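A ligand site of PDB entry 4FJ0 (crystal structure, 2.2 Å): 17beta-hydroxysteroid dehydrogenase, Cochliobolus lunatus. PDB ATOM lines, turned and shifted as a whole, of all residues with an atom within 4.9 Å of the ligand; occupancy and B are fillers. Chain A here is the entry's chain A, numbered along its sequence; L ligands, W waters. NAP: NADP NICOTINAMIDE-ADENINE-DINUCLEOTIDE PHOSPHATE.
O7N of the ligand lies within hydrogen-bond range of N of Thr 200, 2.9 Å away.
The backbone carbonyl oxygen (O) of Gly 25 is in hydrogen-bond range of an oxygen (O3B) of the ligand (2.6 Å).
N6A of the ligand is in hydrogen-bond range of OD1 of Asp 76 (2.9 Å).
The side-chain hydroxyl (OG1) of Thr 202 sits at hydrogen-bond distance from an oxygen (O2N) of the ligand (2.8 Å).
ND2 of Asn 51 lies within hydrogen-bond range of O3X of the ligand, at 2.9 Å.
OG of Ser 52 sits at hydrogen-bond distance from O2X of the ligand.
The side-chain amino group (NZ) of Lys 171 is in hydrogen-bond range of an oxygen (O2D) of the ligand, 2.7 Å away.
The side-chain hydroxyl (OG) of Ser 104 lies within hydrogen-bond range of a nitrogen (N3A) of the ligand (2.8 Å).
The guanidinium group (NE) of Arg 28 is in salt-bridge range of an oxygen (O2X) of the ligand.
The backbone NH (N) of Ser 52 lies within hydrogen-bond range of an oxygen (O1X) of the ligand.
The backbone NH (N) of Ile 77 lies within hydrogen-bond range of a nitrogen (N1A) of the ligand (3.1 Å).
The backbone NH (N) of Asn 51 sits at hydrogen-bond distance from an oxygen (O1X) of the ligand (2.8 Å).
O3D of the ligand is in hydrogen-bond range of O of Asn 103 (2.8 Å).
O1N of the ligand sits at hydrogen-bond distance from N of Ile 30, at 2.9 Å.
O1X of the ligand is in hydrogen-bond range of N of Ala 50, 3.0 Å away.
The backbone carbonyl oxygen (O) of Thr 200 is in hydrogen-bond range of a nitrogen (N7N) of the ligand (3.3 Å).
An oxygen (O2D) of the ligand sits at hydrogen-bond distance from the side-chain hydroxyl (OH) of Tyr 167 (2.6 Å).
N of Gly 25 sits at hydrogen-bond distance from OG of Ser 104 (2.9 Å).
OD1 of Asn 48 sits at hydrogen-bond distance from N of Gly 25, 3.0 Å away.
O of Tyr 49 lies within hydrogen-bond range of N of Ala 75.
OG1 of Thr 202 is in hydrogen-bond range of N of Phe 205, at 3.5 Å.
O of Ala 75 lies within hydrogen-bond range of ND2 of Asn 48 (3.2 Å).
The backbone carbonyl oxygen of Thr 151 sits at hydrogen-bond distance from the side-chain amino group of Lys 171 (3.3 Å).
The side-chain carboxylate (OD2) of Asp 203 is in salt-bridge range of the guanidinium group (NH1) of Arg 28, 2.9 Å away.
OD1 of Asn 103 lies within hydrogen-bond range of N of Gly 31 (3.4 Å).
The backbone carbonyl oxygen (O) of Gly 198 lies close to an oxygen (O7N) of the ligand (3.4 Å).
Gly 29 touches the ligand.
Tyr 49 touches the ligand (CB to O1X, 3.7 Å).
Ala 75 touches the ligand (O to C2A, 3.8 Å).
Arg 78 touches the ligand (NH1 to N6A, 3.6 Å).
Gly 105 touches the ligand.
Leu 126 touches the ligand (CD2 to N7A, 3.4 Å).
Thr 151 touches the ligand.
Ser 152 touches the ligand (O to C6N, 3.4 Å).
OG of Ser 153 touches C5N of the ligand (3.7 Å).
O of Pro 197 touches C5N of the ligand, at 3.2 Å.
Gly 199 touches the ligand (CA to O7N, 3.5 Å).
Asp 203 touches the ligand.
Met 204 touches the ligand.
Of the 36 residues printed, 28 come within 4 Å of the ligand.
The nearest printed residue that does not touch the ligand is Asn 48 (4.01 Å).
Water W5 bridges an oxygen (O1A) of the ligand (2.6 Å) and the backbone carbonyl oxygen (O) of Gly 105 (2.9 Å).
Water W4 lies within hydrogen-bond range of O2A of the ligand (2.6 Å) and OD2 of Asp 203 (2.8 Å).
Water W2 lies within hydrogen-bond range of O1N of the ligand (2.7 Å), ND2 of Asn 103 (2.8 Å), O of Arg 28 (2.8 Å), O of Gly 25 (3.1 Å) and N of Gly 31 (3.1 Å).
Water W3 bridges O2B of the ligand and N of Gly 27.
Water W1 bridges NH1 of Arg 78 (2.8 Å) and N7A of the ligand (2.9 Å).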
ATOM      1  N   GLY A  25      -0.463 -19.364  -9.021  1.00  0.00           N
ATOM      2  CA  GLY A  25      -1.713 -19.448  -8.271  1.00  0.00           C
ATOM      3  C   GLY A  25      -2.884 -18.799  -8.980  1.00  0.00           C
ATOM      4  O   GLY A  25      -3.678 -18.072  -8.355  1.00  0.00           O
ATOM      5  N   SER A  26      -3.006 -19.079 -10.273  1.00  0.00           N
ATOM      6  CA  SER A  26      -4.001 -18.405 -11.098  1.00  0.00           C
ATOM      7  C   SER A  26      -5.188 -19.251 -11.434  1.00  0.00           C
ATOM      8  O   SER A  26      -5.988 -18.863 -12.262  1.00  0.00           O
ATOM      9  CB  SER A  26      -3.359 -17.825 -12.362  1.00  0.00           C
ATOM     10  OG  SER A  26      -2.444 -18.728 -12.939  1.00  0.00           O
ATOM     11  N   GLY A  27      -5.323 -20.399 -10.791  1.00  0.00           N
ATOM     12  CA  GLY A  27      -6.567 -21.171 -10.889  1.00  0.00           C
ATOM     13  C   GLY A  27      -7.790 -20.514 -10.236  1.00  0.00           C
ATOM     14  O   GLY A  27      -8.921 -20.756 -10.637  1.00  0.00           O
ATOM     15  N   ARG A  28      -7.562 -19.697  -9.212  1.00  0.00           N
ATOM     16  CA  ARG A  28      -8.658 -19.010  -8.518  1.00  0.00           C
ATOM     17  C   ARG A  28      -8.196 -17.719  -7.853  1.00  0.00           C
ATOM     18  O   ARG A  28      -7.003 -17.434  -7.807  1.00  0.00           O
ATOM     19  CB  ARG A  28      -9.309 -19.925  -7.469  1.00  0.00           C
ATOM     20  CG  ARG A  28      -8.378 -20.356  -6.339  1.00  0.00           C
ATOM     21  CD  ARG A  28      -8.962 -21.552  -5.565  1.00  0.00           C
ATOM     22  NE  ARG A  28      -7.972 -22.047  -4.628  1.00  0.00           N
ATOM     23  CZ  ARG A  28      -7.842 -21.661  -3.350  1.00  0.00           C
ATOM     24  NH1 ARG A  28      -8.694 -20.806  -2.796  1.00  0.00           N
ATOM     25  NH2 ARG A  28      -6.857 -22.169  -2.626  1.00  0.00           N
ATOM     26  N   GLY A  29      -9.155 -16.951  -7.358  1.00  0.00           N
ATOM     27  CA  GLY A  29      -8.894 -15.749  -6.602  1.00  0.00           C
ATOM     28  C   GLY A  29      -8.311 -14.645  -7.453  1.00  0.00           C
ATOM     29  O   GLY A  29      -8.649 -14.488  -8.626  1.00  0.00           O
ATOM     30  N   ILE A  30      -7.433 -13.857  -6.843  1.00  0.00           N
ATOM     31  CA  ILE A  30      -6.855 -12.728  -7.498  1.00  0.00           C
ATOM     32  C   ILE A  30      -6.069 -13.222  -8.729  1.00  0.00           C
ATOM     33  O   ILE A  30      -6.124 -12.621  -9.784  1.00  0.00           O
ATOM     34  CB  ILE A  30      -5.970 -11.939  -6.543  1.00  0.00           C
ATOM     35  CG1 ILE A  30      -6.844 -11.289  -5.443  1.00  0.00           C
ATOM     36  CG2 ILE A  30      -5.191 -10.897  -7.315  1.00  0.00           C
ATOM     37  CD1 ILE A  30      -6.089 -10.859  -4.209  1.00  0.00           C
ATOM     38  N   GLY A  31      -5.333 -14.319  -8.566  1.00  0.00           N
ATOM     39  CA  GLY A  31      -4.516 -14.832  -9.651  1.00  0.00           C
ATOM     40  C   GLY A  31      -5.335 -15.195 -10.878  1.00  0.00           C
ATOM     41  O   GLY A  31      -4.910 -14.950 -12.000  1.00  0.00           O
ATOM     42  N   ASN A  48      -0.469 -21.192 -13.697  1.00  0.00           N
ATOM     43  CA  ASN A  48       0.054 -22.116 -12.709  1.00  0.00           C
ATOM     44  C   ASN A  48      -0.979 -22.359 -11.596  1.00  0.00           C
ATOM     45  O   ASN A  48      -1.688 -21.449 -11.196  1.00  0.00           O
ATOM     46  CB  ASN A  48       1.357 -21.601 -12.114  1.00  0.00           C
ATOM     47  CG  ASN A  48       1.669 -22.212 -10.756  1.00  0.00           C
ATOM     48  OD1 ASN A  48       1.482 -21.562  -9.734  1.00  0.00           O
ATOM     49  ND2 ASN A  48       2.085 -23.475 -10.745  1.00  0.00           N
ATOM     50  N   TYR A  49      -1.063 -23.592 -11.141  1.00  0.00           N
ATOM     51  CA  TYR A  49      -1.849 -23.946  -9.961  1.00  0.00           C
ATOM     52  C   TYR A  49      -1.092 -25.015  -9.186  1.00  0.00           C
ATOM     53  O   TYR A  49      -0.153 -25.624  -9.718  1.00  0.00           O
ATOM     54  CB  TYR A  49      -3.215 -24.508 -10.360  1.00  0.00           C
ATOM     55  CG  TYR A  49      -3.131 -25.797 -11.120  1.00  0.00           C
ATOM     56  CD1 TYR A  49      -2.809 -25.796 -12.470  1.00  0.00           C
ATOM     57  CD2 TYR A  49      -3.364 -27.029 -10.495  1.00  0.00           C
ATOM     58  CE1 TYR A  49      -2.720 -26.979 -13.182  1.00  0.00           C
ATOM     59  CE2 TYR A  49      -3.266 -28.224 -11.191  1.00  0.00           C
ATOM     60  CZ  TYR A  49      -2.953 -28.179 -12.538  1.00  0.00           C
ATOM     61  OH  TYR A  49      -2.857 -29.321 -13.271  1.00  0.00           O
ATOM     62  N   ALA A  50      -1.508 -25.247  -7.946  1.00  0.00           N
ATOM     63  CA  ALA A  50      -0.943 -26.314  -7.119  1.00  0.00           C
ATOM     64  C   ALA A  50      -1.956 -27.429  -6.833  1.00  0.00           C
ATOM     65  O   ALA A  50      -1.595 -28.604  -6.820  1.00  0.00           O
ATOM     66  CB  ALA A  50      -0.407 -25.736  -5.821  1.00  0.00           C
ATOM     67  N   ASN A  51      -3.207 -27.052  -6.576  1.00  0.00           N
ATOM     68  CA  ASN A  51      -4.266 -27.997  -6.236  1.00  0.00           C
ATOM     69  C   ASN A  51      -5.540 -27.861  -7.068  1.00  0.00           C
ATOM     70  O   ASN A  51      -6.231 -28.834  -7.307  1.00  0.00           O
ATOM     71  CB  ASN A  51      -4.648 -27.829  -4.758  1.00  0.00           C
ATOM     72  CG  ASN A  51      -3.457 -27.978  -3.822  1.00  0.00           C
ATOM     73  OD1 ASN A  51      -3.001 -29.080  -3.563  1.00  0.00           O
ATOM     74  ND2 ASN A  51      -2.940 -26.861  -3.349  1.00  0.00           N
ATOM     75  N   SER A  52      -5.865 -26.639  -7.503  1.00  0.00           N
ATOM     76  CA  SER A  52      -7.145 -26.346  -8.134  1.00  0.00           C
ATOM     77  C   SER A  52      -7.104 -26.642  -9.636  1.00  0.00           C
ATOM     78  O   SER A  52      -7.151 -25.739 -10.463  1.00  0.00           O
ATOM     79  CB  SER A  52      -7.522 -24.890  -7.880  1.00  0.00           C
ATOM     80  OG  SER A  52      -7.424 -24.567  -6.508  1.00  0.00           O
ATOM     81  N   ALA A  75       2.533 -26.701 -10.432  1.00  0.00           N
ATOM     82  CA  ALA A  75       3.802 -26.574  -9.737  1.00  0.00           C
ATOM     83  C   ALA A  75       3.547 -26.058  -8.342  1.00  0.00           C
ATOM     84  O   ALA A  75       2.821 -25.095  -8.145  1.00  0.00           O
ATOM     85  CB  ALA A  75       4.753 -25.610 -10.474  1.00  0.00           C
ATOM     86  N   ASP A  76       4.172 -26.721  -7.373  1.00  0.00           N
ATOM     87  CA  ASP A  76       4.133 -26.288  -5.981  1.00  0.00           C
ATOM     88  C   ASP A  76       5.255 -25.248  -5.792  1.00  0.00           C
ATOM     89  O   ASP A  76       6.441 -25.573  -5.805  1.00  0.00           O
ATOM     90  CB  ASP A  76       4.332 -27.494  -5.061  1.00  0.00           C
ATOM     91  CG  ASP A  76       4.363 -27.108  -3.578  1.00  0.00           C
ATOM     92  OD1 ASP A  76       4.242 -25.911  -3.203  1.00  0.00           O
ATOM     93  OD2 ASP A  76       4.540 -28.048  -2.771  1.00  0.00           O
ATOM     94  N   ILE A  77       4.845 -23.990  -5.607  1.00  0.00           N
ATOM     95  CA  ILE A  77       5.786 -22.870  -5.546  1.00  0.00           C
ATOM     96  C   ILE A  77       6.636 -22.880  -4.257  1.00  0.00           C
ATOM     97  O   ILE A  77       7.612 -22.119  -4.162  1.00  0.00           O
ATOM     98  CB  ILE A  77       5.039 -21.527  -5.745  1.00  0.00           C
ATOM     99  CG1 ILE A  77       4.393 -21.465  -7.126  1.00  0.00           C
ATOM    100  CG2 ILE A  77       5.942 -20.301  -5.555  1.00  0.00           C
ATOM    101  CD1 ILE A  77       5.366 -21.502  -8.295  1.00  0.00           C
ATOM    102  N   ARG A  78       6.304 -23.728  -3.282  1.00  0.00           N
ATOM    103  CA  ARG A  78       7.185 -23.963  -2.142  1.00  0.00           C
ATOM    104  C   ARG A  78       8.465 -24.713  -2.547  1.00  0.00           C
ATOM    105  O   ARG A  78       9.463 -24.645  -1.836  1.00  0.00           O
ATOM    106  CB  ARG A  78       6.484 -24.768  -1.035  1.00  0.00           C
ATOM    107  CG  ARG A  78       5.400 -23.999  -0.321  1.00  0.00           C
ATOM    108  CD  ARG A  78       4.979 -24.671   0.978  1.00  0.00           C
ATOM    109  NE  ARG A  78       4.054 -23.799   1.716  1.00  0.00           N
ATOM    110  CZ  ARG A  78       2.731 -23.794   1.589  1.00  0.00           C
ATOM    111  NH1 ARG A  78       2.125 -24.625   0.757  1.00  0.00           N
ATOM    112  NH2 ARG A  78       2.002 -22.947   2.311  1.00  0.00           N
ATOM    113  N   ASN A 103       1.742 -14.475  -7.456  1.00  0.00           N
ATOM    114  CA  ASN A 103       0.496 -14.218  -6.751  1.00  0.00           C
ATOM    115  C   ASN A 103       0.204 -15.226  -5.626  1.00  0.00           C
ATOM    116  O   ASN A 103      -0.541 -14.929  -4.695  1.00  0.00           O
ATOM    117  CB  ASN A 103      -0.624 -14.220  -7.770  1.00  0.00           C
ATOM    118  CG  ASN A 103      -1.978 -14.423  -7.162  1.00  0.00           C
ATOM    119  OD1 ASN A 103      -2.611 -13.469  -6.689  1.00  0.00           O
ATOM    120  ND2 ASN A 103      -2.443 -15.690  -7.149  1.00  0.00           N
ATOM    121  N   SER A 104       0.760 -16.417  -5.722  1.00  0.00           N
ATOM    122  CA  SER A 104       0.477 -17.491  -4.753  1.00  0.00           C
ATOM    123  C   SER A 104       0.785 -17.053  -3.320  1.00  0.00           C
ATOM    124  O   SER A 104       1.791 -16.408  -3.073  1.00  0.00           O
ATOM    125  CB  SER A 104       1.257 -18.741  -5.130  1.00  0.00           C
ATOM    126  OG  SER A 104       0.772 -19.258  -6.378  1.00  0.00           O
ATOM    127  N   GLY A 105      -0.128 -17.324  -2.401  1.00  0.00           N
ATOM    128  CA  GLY A 105       0.051 -16.961  -1.001  1.00  0.00           C
ATOM    129  C   GLY A 105      -0.970 -17.615  -0.106  1.00  0.00           C
ATOM    130  O   GLY A 105      -2.027 -18.046  -0.591  1.00  0.00           O
ATOM    131  N   VAL A 106      -0.635 -17.726   1.184  1.00  0.00           N
ATOM    132  CA  VAL A 106      -1.547 -18.202   2.215  1.00  0.00           C
ATOM    133  C   VAL A 106      -1.582 -17.165   3.340  1.00  0.00           C
ATOM    134  O   VAL A 106      -0.624 -16.388   3.526  1.00  0.00           O
ATOM    135  CB  VAL A 106      -1.095 -19.550   2.816  1.00  0.00           C
ATOM    136  CG1 VAL A 106      -1.279 -20.687   1.814  1.00  0.00           C
ATOM    137  CG2 VAL A 106       0.366 -19.428   3.270  1.00  0.00           C
ATOM    138  N   LEU A 126       6.000 -20.093   1.230  1.00  0.00           N
ATOM    139  CA  LEU A 126       5.223 -19.695   0.055  1.00  0.00           C
ATOM    140  C   LEU A 126       5.255 -18.180  -0.168  1.00  0.00           C
ATOM    141  O   LEU A 126       5.603 -17.738  -1.266  1.00  0.00           O
ATOM    142  CB  LEU A 126       3.784 -20.178   0.151  1.00  0.00           C
ATOM    143  CG  LEU A 126       2.951 -19.978  -1.142  1.00  0.00           C
ATOM    144  CD1 LEU A 126       3.552 -20.626  -2.386  1.00  0.00           C
ATOM    145  CD2 LEU A 126       1.538 -20.472  -0.896  1.00  0.00           C
ATOM    146  N   ASN A 127       4.931 -17.401   0.859  1.00  0.00           N
ATOM    147  CA  ASN A 127       4.710 -15.972   0.684  1.00  0.00           C
ATOM    148  C   ASN A 127       5.996 -15.178   0.404  1.00  0.00           C
ATOM    149  O   ASN A 127       5.955 -14.132  -0.229  1.00  0.00           O
ATOM    150  CB  ASN A 127       4.024 -15.361   1.921  1.00  0.00           C
ATOM    151  CG  ASN A 127       2.602 -15.840   2.109  1.00  0.00           C
ATOM    152  OD1 ASN A 127       2.147 -16.746   1.432  1.00  0.00           O
ATOM    153  ND2 ASN A 127       1.889 -15.222   3.038  1.00  0.00           N
ATOM    154  N   THR A 151       3.268 -10.090  -5.062  1.00  0.00           N
ATOM    155  CA  THR A 151       2.089  -9.743  -4.280  1.00  0.00           C
ATOM    156  C   THR A 151       2.451  -9.558  -2.809  1.00  0.00           C
ATOM    157  O   THR A 151       3.063 -10.427  -2.187  1.00  0.00           O
ATOM    158  CB  THR A 151       0.970 -10.772  -4.456  1.00  0.00           C
ATOM    159  OG1 THR A 151       0.732 -10.976  -5.868  1.00  0.00           O
ATOM    160  CG2 THR A 151      -0.349 -10.268  -3.809  1.00  0.00           C
ATOM    161  N   SER A 152       2.085  -8.397  -2.290  1.00  0.00           N
ATOM    162  CA  SER A 152       2.302  -8.066  -0.904  1.00  0.00           C
ATOM    163  C   SER A 152       0.906  -7.918  -0.288  1.00  0.00           C
ATOM    164  O   SER A 152      -0.008  -8.659  -0.649  1.00  0.00           O
ATOM    165  CB  SER A 152       3.134  -6.776  -0.779  1.00  0.00           C
ATOM    166  OG  SER A 152       3.376  -6.443   0.583  1.00  0.00           O
ATOM    167  N   SER A 153       0.735  -6.953   0.608  1.00  0.00           N
ATOM    168  CA  SER A 153      -0.518  -6.784   1.322  1.00  0.00           C
ATOM    169  C   SER A 153      -0.545  -5.434   2.007  1.00  0.00           C
ATOM    170  O   SER A 153       0.483  -4.960   2.424  1.00  0.00           O
ATOM    171  CB  SER A 153      -0.630  -7.891   2.381  1.00  0.00           C
ATOM    172  OG  SER A 153      -1.705  -7.654   3.275  1.00  0.00           O
ATOM    173  N   TYR A 167       1.981 -13.161   8.916  1.00  0.00           N
ATOM    174  CA  TYR A 167       1.611 -12.787   7.566  1.00  0.00           C
ATOM    175  C   TYR A 167       2.116 -11.383   7.186  1.00  0.00           C
ATOM    176  O   TYR A 167       2.636 -11.183   6.100  1.00  0.00           O
ATOM    177  CB  TYR A 167       0.111 -12.831   7.413  1.00  0.00           C
ATOM    178  CG  TYR A 167      -0.376 -12.484   6.033  1.00  0.00           C
ATOM    179  CD1 TYR A 167      -0.348 -13.419   5.010  1.00  0.00           C
ATOM    180  CD2 TYR A 167      -0.899 -11.229   5.763  1.00  0.00           C
ATOM    181  CE1 TYR A 167      -0.846 -13.113   3.746  1.00  0.00           C
ATOM    182  CE2 TYR A 167      -1.393 -10.896   4.506  1.00  0.00           C
ATOM    183  CZ  TYR A 167      -1.356 -11.828   3.493  1.00  0.00           C
ATOM    184  OH  TYR A 167      -1.875 -11.498   2.260  1.00  0.00           O
ATOM    185  N   LYS A 171       4.905 -10.431   4.041  1.00  0.00           N
ATOM    186  CA  LYS A 171       4.681  -9.510   2.953  1.00  0.00           C
ATOM    187  C   LYS A 171       5.551  -8.252   3.063  1.00  0.00           C
ATOM    188  O   LYS A 171       5.867  -7.644   2.056  1.00  0.00           O
ATOM    189  CB  LYS A 171       3.186  -9.186   2.856  1.00  0.00           C
ATOM    190  CG  LYS A 171       2.303 -10.399   2.572  1.00  0.00           C
ATOM    191  CD  LYS A 171       2.853 -11.267   1.443  1.00  0.00           C
ATOM    192  CE  LYS A 171       1.849 -12.289   0.905  1.00  0.00           C
ATOM    193  NZ  LYS A 171       0.875 -11.714  -0.065  1.00  0.00           N
ATOM    194  N   PRO A 197      -2.794  -5.593  -1.990  1.00  0.00           N
ATOM    195  CA  PRO A 197      -4.223  -5.404  -1.851  1.00  0.00           C
ATOM    196  C   PRO A 197      -4.650  -5.323  -0.410  1.00  0.00           C
ATOM    197  O   PRO A 197      -3.990  -5.894   0.464  1.00  0.00           O
ATOM    198  CB  PRO A 197      -4.827  -6.659  -2.483  1.00  0.00           C
ATOM    199  CG  PRO A 197      -3.710  -7.304  -3.242  1.00  0.00           C
ATOM    200  CD  PRO A 197      -2.455  -6.915  -2.527  1.00  0.00           C
ATOM    201  N   GLY A 198      -5.734  -4.589  -0.146  1.00  0.00           N
ATOM    202  CA  GLY A 198      -6.449  -4.712   1.097  1.00  0.00           C
ATOM    203  C   GLY A 198      -7.438  -5.863   0.951  1.00  0.00           C
ATOM    204  O   GLY A 198      -7.270  -6.711   0.087  1.00  0.00           O
ATOM    205  N   GLY A 199      -8.449  -5.884   1.785  1.00  0.00           N
ATOM    206  CA  GLY A 199      -9.489  -6.909   1.723  1.00  0.00           C
ATOM    207  C   GLY A 199     -10.147  -6.964   0.376  1.00  0.00           C
ATOM    208  O   GLY A 199     -10.761  -6.007  -0.065  1.00  0.00           O
ATOM    209  N   THR A 200      -9.967  -8.088  -0.303  1.00  0.00           N
ATOM    210  CA  THR A 200     -10.460  -8.292  -1.653  1.00  0.00           C
ATOM    211  C   THR A 200     -11.287  -9.584  -1.591  1.00  0.00           C
ATOM    212  O   THR A 200     -10.805 -10.573  -1.064  1.00  0.00           O
ATOM    213  CB  THR A 200      -9.281  -8.428  -2.630  1.00  0.00           C
ATOM    214  OG1 THR A 200      -8.390  -7.316  -2.479  1.00  0.00           O
ATOM    215  CG2 THR A 200      -9.778  -8.473  -4.084  1.00  0.00           C
ATOM    216  N   THR A 202     -12.425 -12.914  -2.062  1.00  0.00           N
ATOM    217  CA  THR A 202     -11.939 -14.179  -2.618  1.00  0.00           C
ATOM    218  C   THR A 202     -12.158 -15.232  -1.506  1.00  0.00           C
ATOM    219  O   THR A 202     -12.709 -14.914  -0.474  1.00  0.00           O
ATOM    220  CB  THR A 202     -10.423 -14.142  -2.919  1.00  0.00           C
ATOM    221  OG1 THR A 202      -9.702 -13.946  -1.701  1.00  0.00           O
ATOM    222  CG2 THR A 202     -10.064 -13.018  -3.897  1.00  0.00           C
ATOM    223  N   ASP A 203     -11.683 -16.459  -1.704  1.00  0.00           N
ATOM    224  CA  ASP A 203     -11.695 -17.466  -0.634  1.00  0.00           C
ATOM    225  C   ASP A 203     -10.932 -16.966   0.608  1.00  0.00           C
ATOM    226  O   ASP A 203     -11.362 -17.187   1.726  1.00  0.00           O
ATOM    227  CB  ASP A 203     -11.096 -18.802  -1.121  1.00  0.00           C
ATOM    228  CG  ASP A 203     -11.971 -19.482  -2.163  1.00  0.00           C
ATOM    229  OD1 ASP A 203     -13.201 -19.573  -1.932  1.00  0.00           O
ATOM    230  OD2 ASP A 203     -11.446 -19.944  -3.220  1.00  0.00           O
ATOM    231  N   MET A 204      -9.798 -16.291   0.393  1.00  0.00           N
ATOM    232  CA  MET A 204      -8.998 -15.763   1.500  1.00  0.00           C
ATOM    233  C   MET A 204      -9.734 -14.683   2.327  1.00  0.00           C
ATOM    234  O   MET A 204      -9.572 -14.582   3.545  1.00  0.00           O
ATOM    235  CB  MET A 204      -7.679 -15.193   0.976  1.00  0.00           C
ATOM    236  CG  MET A 204      -6.748 -14.672   2.060  1.00  0.00           C
ATOM    237  SD  MET A 204      -5.149 -14.100   1.482  1.00  0.00           S
ATOM    238  CE  MET A 204      -4.387 -15.643   0.934  1.00  0.00           C
ATOM    239  N   PHE A 205     -10.578 -13.889   1.669  1.00  0.00           N
ATOM    240  CA  PHE A 205     -11.335 -12.853   2.362  1.00  0.00           C
ATOM    241  C   PHE A 205     -12.130 -13.425   3.537  1.00  0.00           C
ATOM    242  O   PHE A 205     -12.227 -12.813   4.598  1.00  0.00           O
ATOM    243  CB  PHE A 205     -12.266 -12.138   1.392  1.00  0.00           C
ATOM    244  CG  PHE A 205     -13.059 -11.000   1.993  1.00  0.00           C
ATOM    245  CD1 PHE A 205     -12.519  -9.705   2.060  1.00  0.00           C
ATOM    246  CD2 PHE A 205     -14.334 -11.198   2.475  1.00  0.00           C
ATOM    247  CE1 PHE A 205     -13.246  -8.650   2.596  1.00  0.00           C
ATOM    248  CE2 PHE A 205     -15.076 -10.158   3.020  1.00  0.00           C
ATOM    249  CZ  PHE A 205     -14.522  -8.880   3.090  1.00  0.00           C
ATOM    250  N   VAL A 208      -9.954 -13.725   6.488  1.00  0.00           N
ATOM    251  CA  VAL A 208      -9.470 -12.494   7.112  1.00  0.00           C
ATOM    252  C   VAL A 208     -10.555 -11.601   7.713  1.00  0.00           C
ATOM    253  O   VAL A 208     -10.240 -10.789   8.586  1.00  0.00           O
ATOM    254  CB  VAL A 208      -8.618 -11.617   6.158  1.00  0.00           C
ATOM    255  CG1 VAL A 208      -7.464 -12.436   5.576  1.00  0.00           C
ATOM    256  CG2 VAL A 208      -9.475 -10.972   5.074  1.00  0.00           C
HETATM  257  PA  NAP L   1      -6.803 -17.378  -2.248  1.00  0.00           P
HETATM  258  O1A NAP L   1      -6.520 -18.154  -1.035  1.00  0.00           O
HETATM  259  O2A NAP L   1      -8.180 -17.344  -2.756  1.00  0.00           O
HETATM  260  O5B NAP L   1      -5.888 -18.013  -3.402  1.00  0.00           O
HETATM  261  C5B NAP L   1      -4.641 -18.618  -3.091  1.00  0.00           C
HETATM  262  C4B NAP L   1      -3.891 -18.849  -4.382  1.00  0.00           C
HETATM  263  O4B NAP L   1      -2.602 -19.333  -4.024  1.00  0.00           O
HETATM  264  C3B NAP L   1      -4.582 -19.987  -5.116  1.00  0.00           C
HETATM  265  O3B NAP L   1      -4.366 -19.813  -6.508  1.00  0.00           O
HETATM  266  C2B NAP L   1      -3.779 -21.173  -4.663  1.00  0.00           C
HETATM  267  O2B NAP L   1      -3.819 -22.136  -5.682  1.00  0.00           O
HETATM  268  C1B NAP L   1      -2.412 -20.537  -4.684  1.00  0.00           C
HETATM  269  N9A NAP L   1      -1.511 -21.393  -3.957  1.00  0.00           N
HETATM  270  C8A NAP L   1      -1.646 -21.811  -2.698  1.00  0.00           C
HETATM  271  N7A NAP L   1      -0.636 -22.618  -2.383  1.00  0.00           N
HETATM  272  C5A NAP L   1       0.154 -22.720  -3.447  1.00  0.00           C
HETATM  273  C6A NAP L   1       1.339 -23.404  -3.703  1.00  0.00           C
HETATM  274  N6A NAP L   1       1.955 -24.183  -2.795  1.00  0.00           N
HETATM  275  N1A NAP L   1       1.871 -23.275  -4.925  1.00  0.00           N
HETATM  276  C2A NAP L   1       1.280 -22.512  -5.841  1.00  0.00           C
HETATM  277  N3A NAP L   1       0.139 -21.864  -5.644  1.00  0.00           N
HETATM  278  C4A NAP L   1      -0.432 -21.957  -4.458  1.00  0.00           C
HETATM  279  O3  NAP L   1      -6.135 -15.977  -2.057  1.00  0.00           O
HETATM  280  PN  NAP L   1      -6.146 -14.643  -2.920  1.00  0.00           P
HETATM  281  O1N NAP L   1      -6.339 -14.854  -4.361  1.00  0.00           O
HETATM  282  O2N NAP L   1      -6.948 -13.617  -2.191  1.00  0.00           O
HETATM  283  O5D NAP L   1      -4.656 -14.295  -2.714  1.00  0.00           O
HETATM  284  C5D NAP L   1      -3.800 -13.827  -3.770  1.00  0.00           C
HETATM  285  C4D NAP L   1      -2.560 -13.162  -3.208  1.00  0.00           C
HETATM  286  O4D NAP L   1      -3.086 -11.925  -2.664  1.00  0.00           O
HETATM  287  C3D NAP L   1      -1.874 -13.885  -2.034  1.00  0.00           C
HETATM  288  O3D NAP L   1      -0.452 -13.704  -2.177  1.00  0.00           O
HETATM  289  C2D NAP L   1      -2.373 -13.139  -0.800  1.00  0.00           C
HETATM  290  O2D NAP L   1      -1.389 -13.092   0.242  1.00  0.00           O
HETATM  291  C1D NAP L   1      -2.490 -11.752  -1.369  1.00  0.00           C
HETATM  292  N1N NAP L   1      -3.494 -10.956  -0.661  1.00  0.00           N
HETATM  293  C2N NAP L   1      -4.852 -11.342  -0.647  1.00  0.00           C
HETATM  294  C3N NAP L   1      -5.772 -10.555   0.047  1.00  0.00           C
HETATM  295  C7N NAP L   1      -7.261 -10.856   0.094  1.00  0.00           C
HETATM  296  O7N NAP L   1      -8.019 -10.001   0.801  1.00  0.00           O
HETATM  297  N7N NAP L   1      -7.758 -11.779  -0.728  1.00  0.00           N
HETATM  298  C4N NAP L   1      -5.377  -9.423   0.710  1.00  0.00           C
HETATM  299  C5N NAP L   1      -4.046  -9.035   0.701  1.00  0.00           C
HETATM  300  C6N NAP L   1      -3.110  -9.793   0.002  1.00  0.00           C
HETATM  301  P2B NAP L   1      -4.286 -23.608  -5.494  1.00  0.00           P
HETATM  302  O1X NAP L   1      -4.047 -24.362  -6.721  1.00  0.00           O
HETATM  303  O2X NAP L   1      -5.754 -23.635  -5.051  1.00  0.00           O
HETATM  304  O3X NAP L   1      -3.438 -24.213  -4.324  1.00  0.00           O
HETATM  305  O   HOH W   1      -0.497 -24.349  -0.055  1.00  0.00           O
HETATM  306  O   HOH W   2      -4.987 -16.302  -6.234  1.00  0.00           O
HETATM  307  O   HOH W   3      -4.491 -22.063  -8.428  1.00  0.00           O
HETATM  308  O   HOH W   4     -10.390 -17.551  -4.089  1.00  0.00           O
HETATM  309  O   HOH W   5      -4.570 -19.278   0.240  1.00  0.00           O
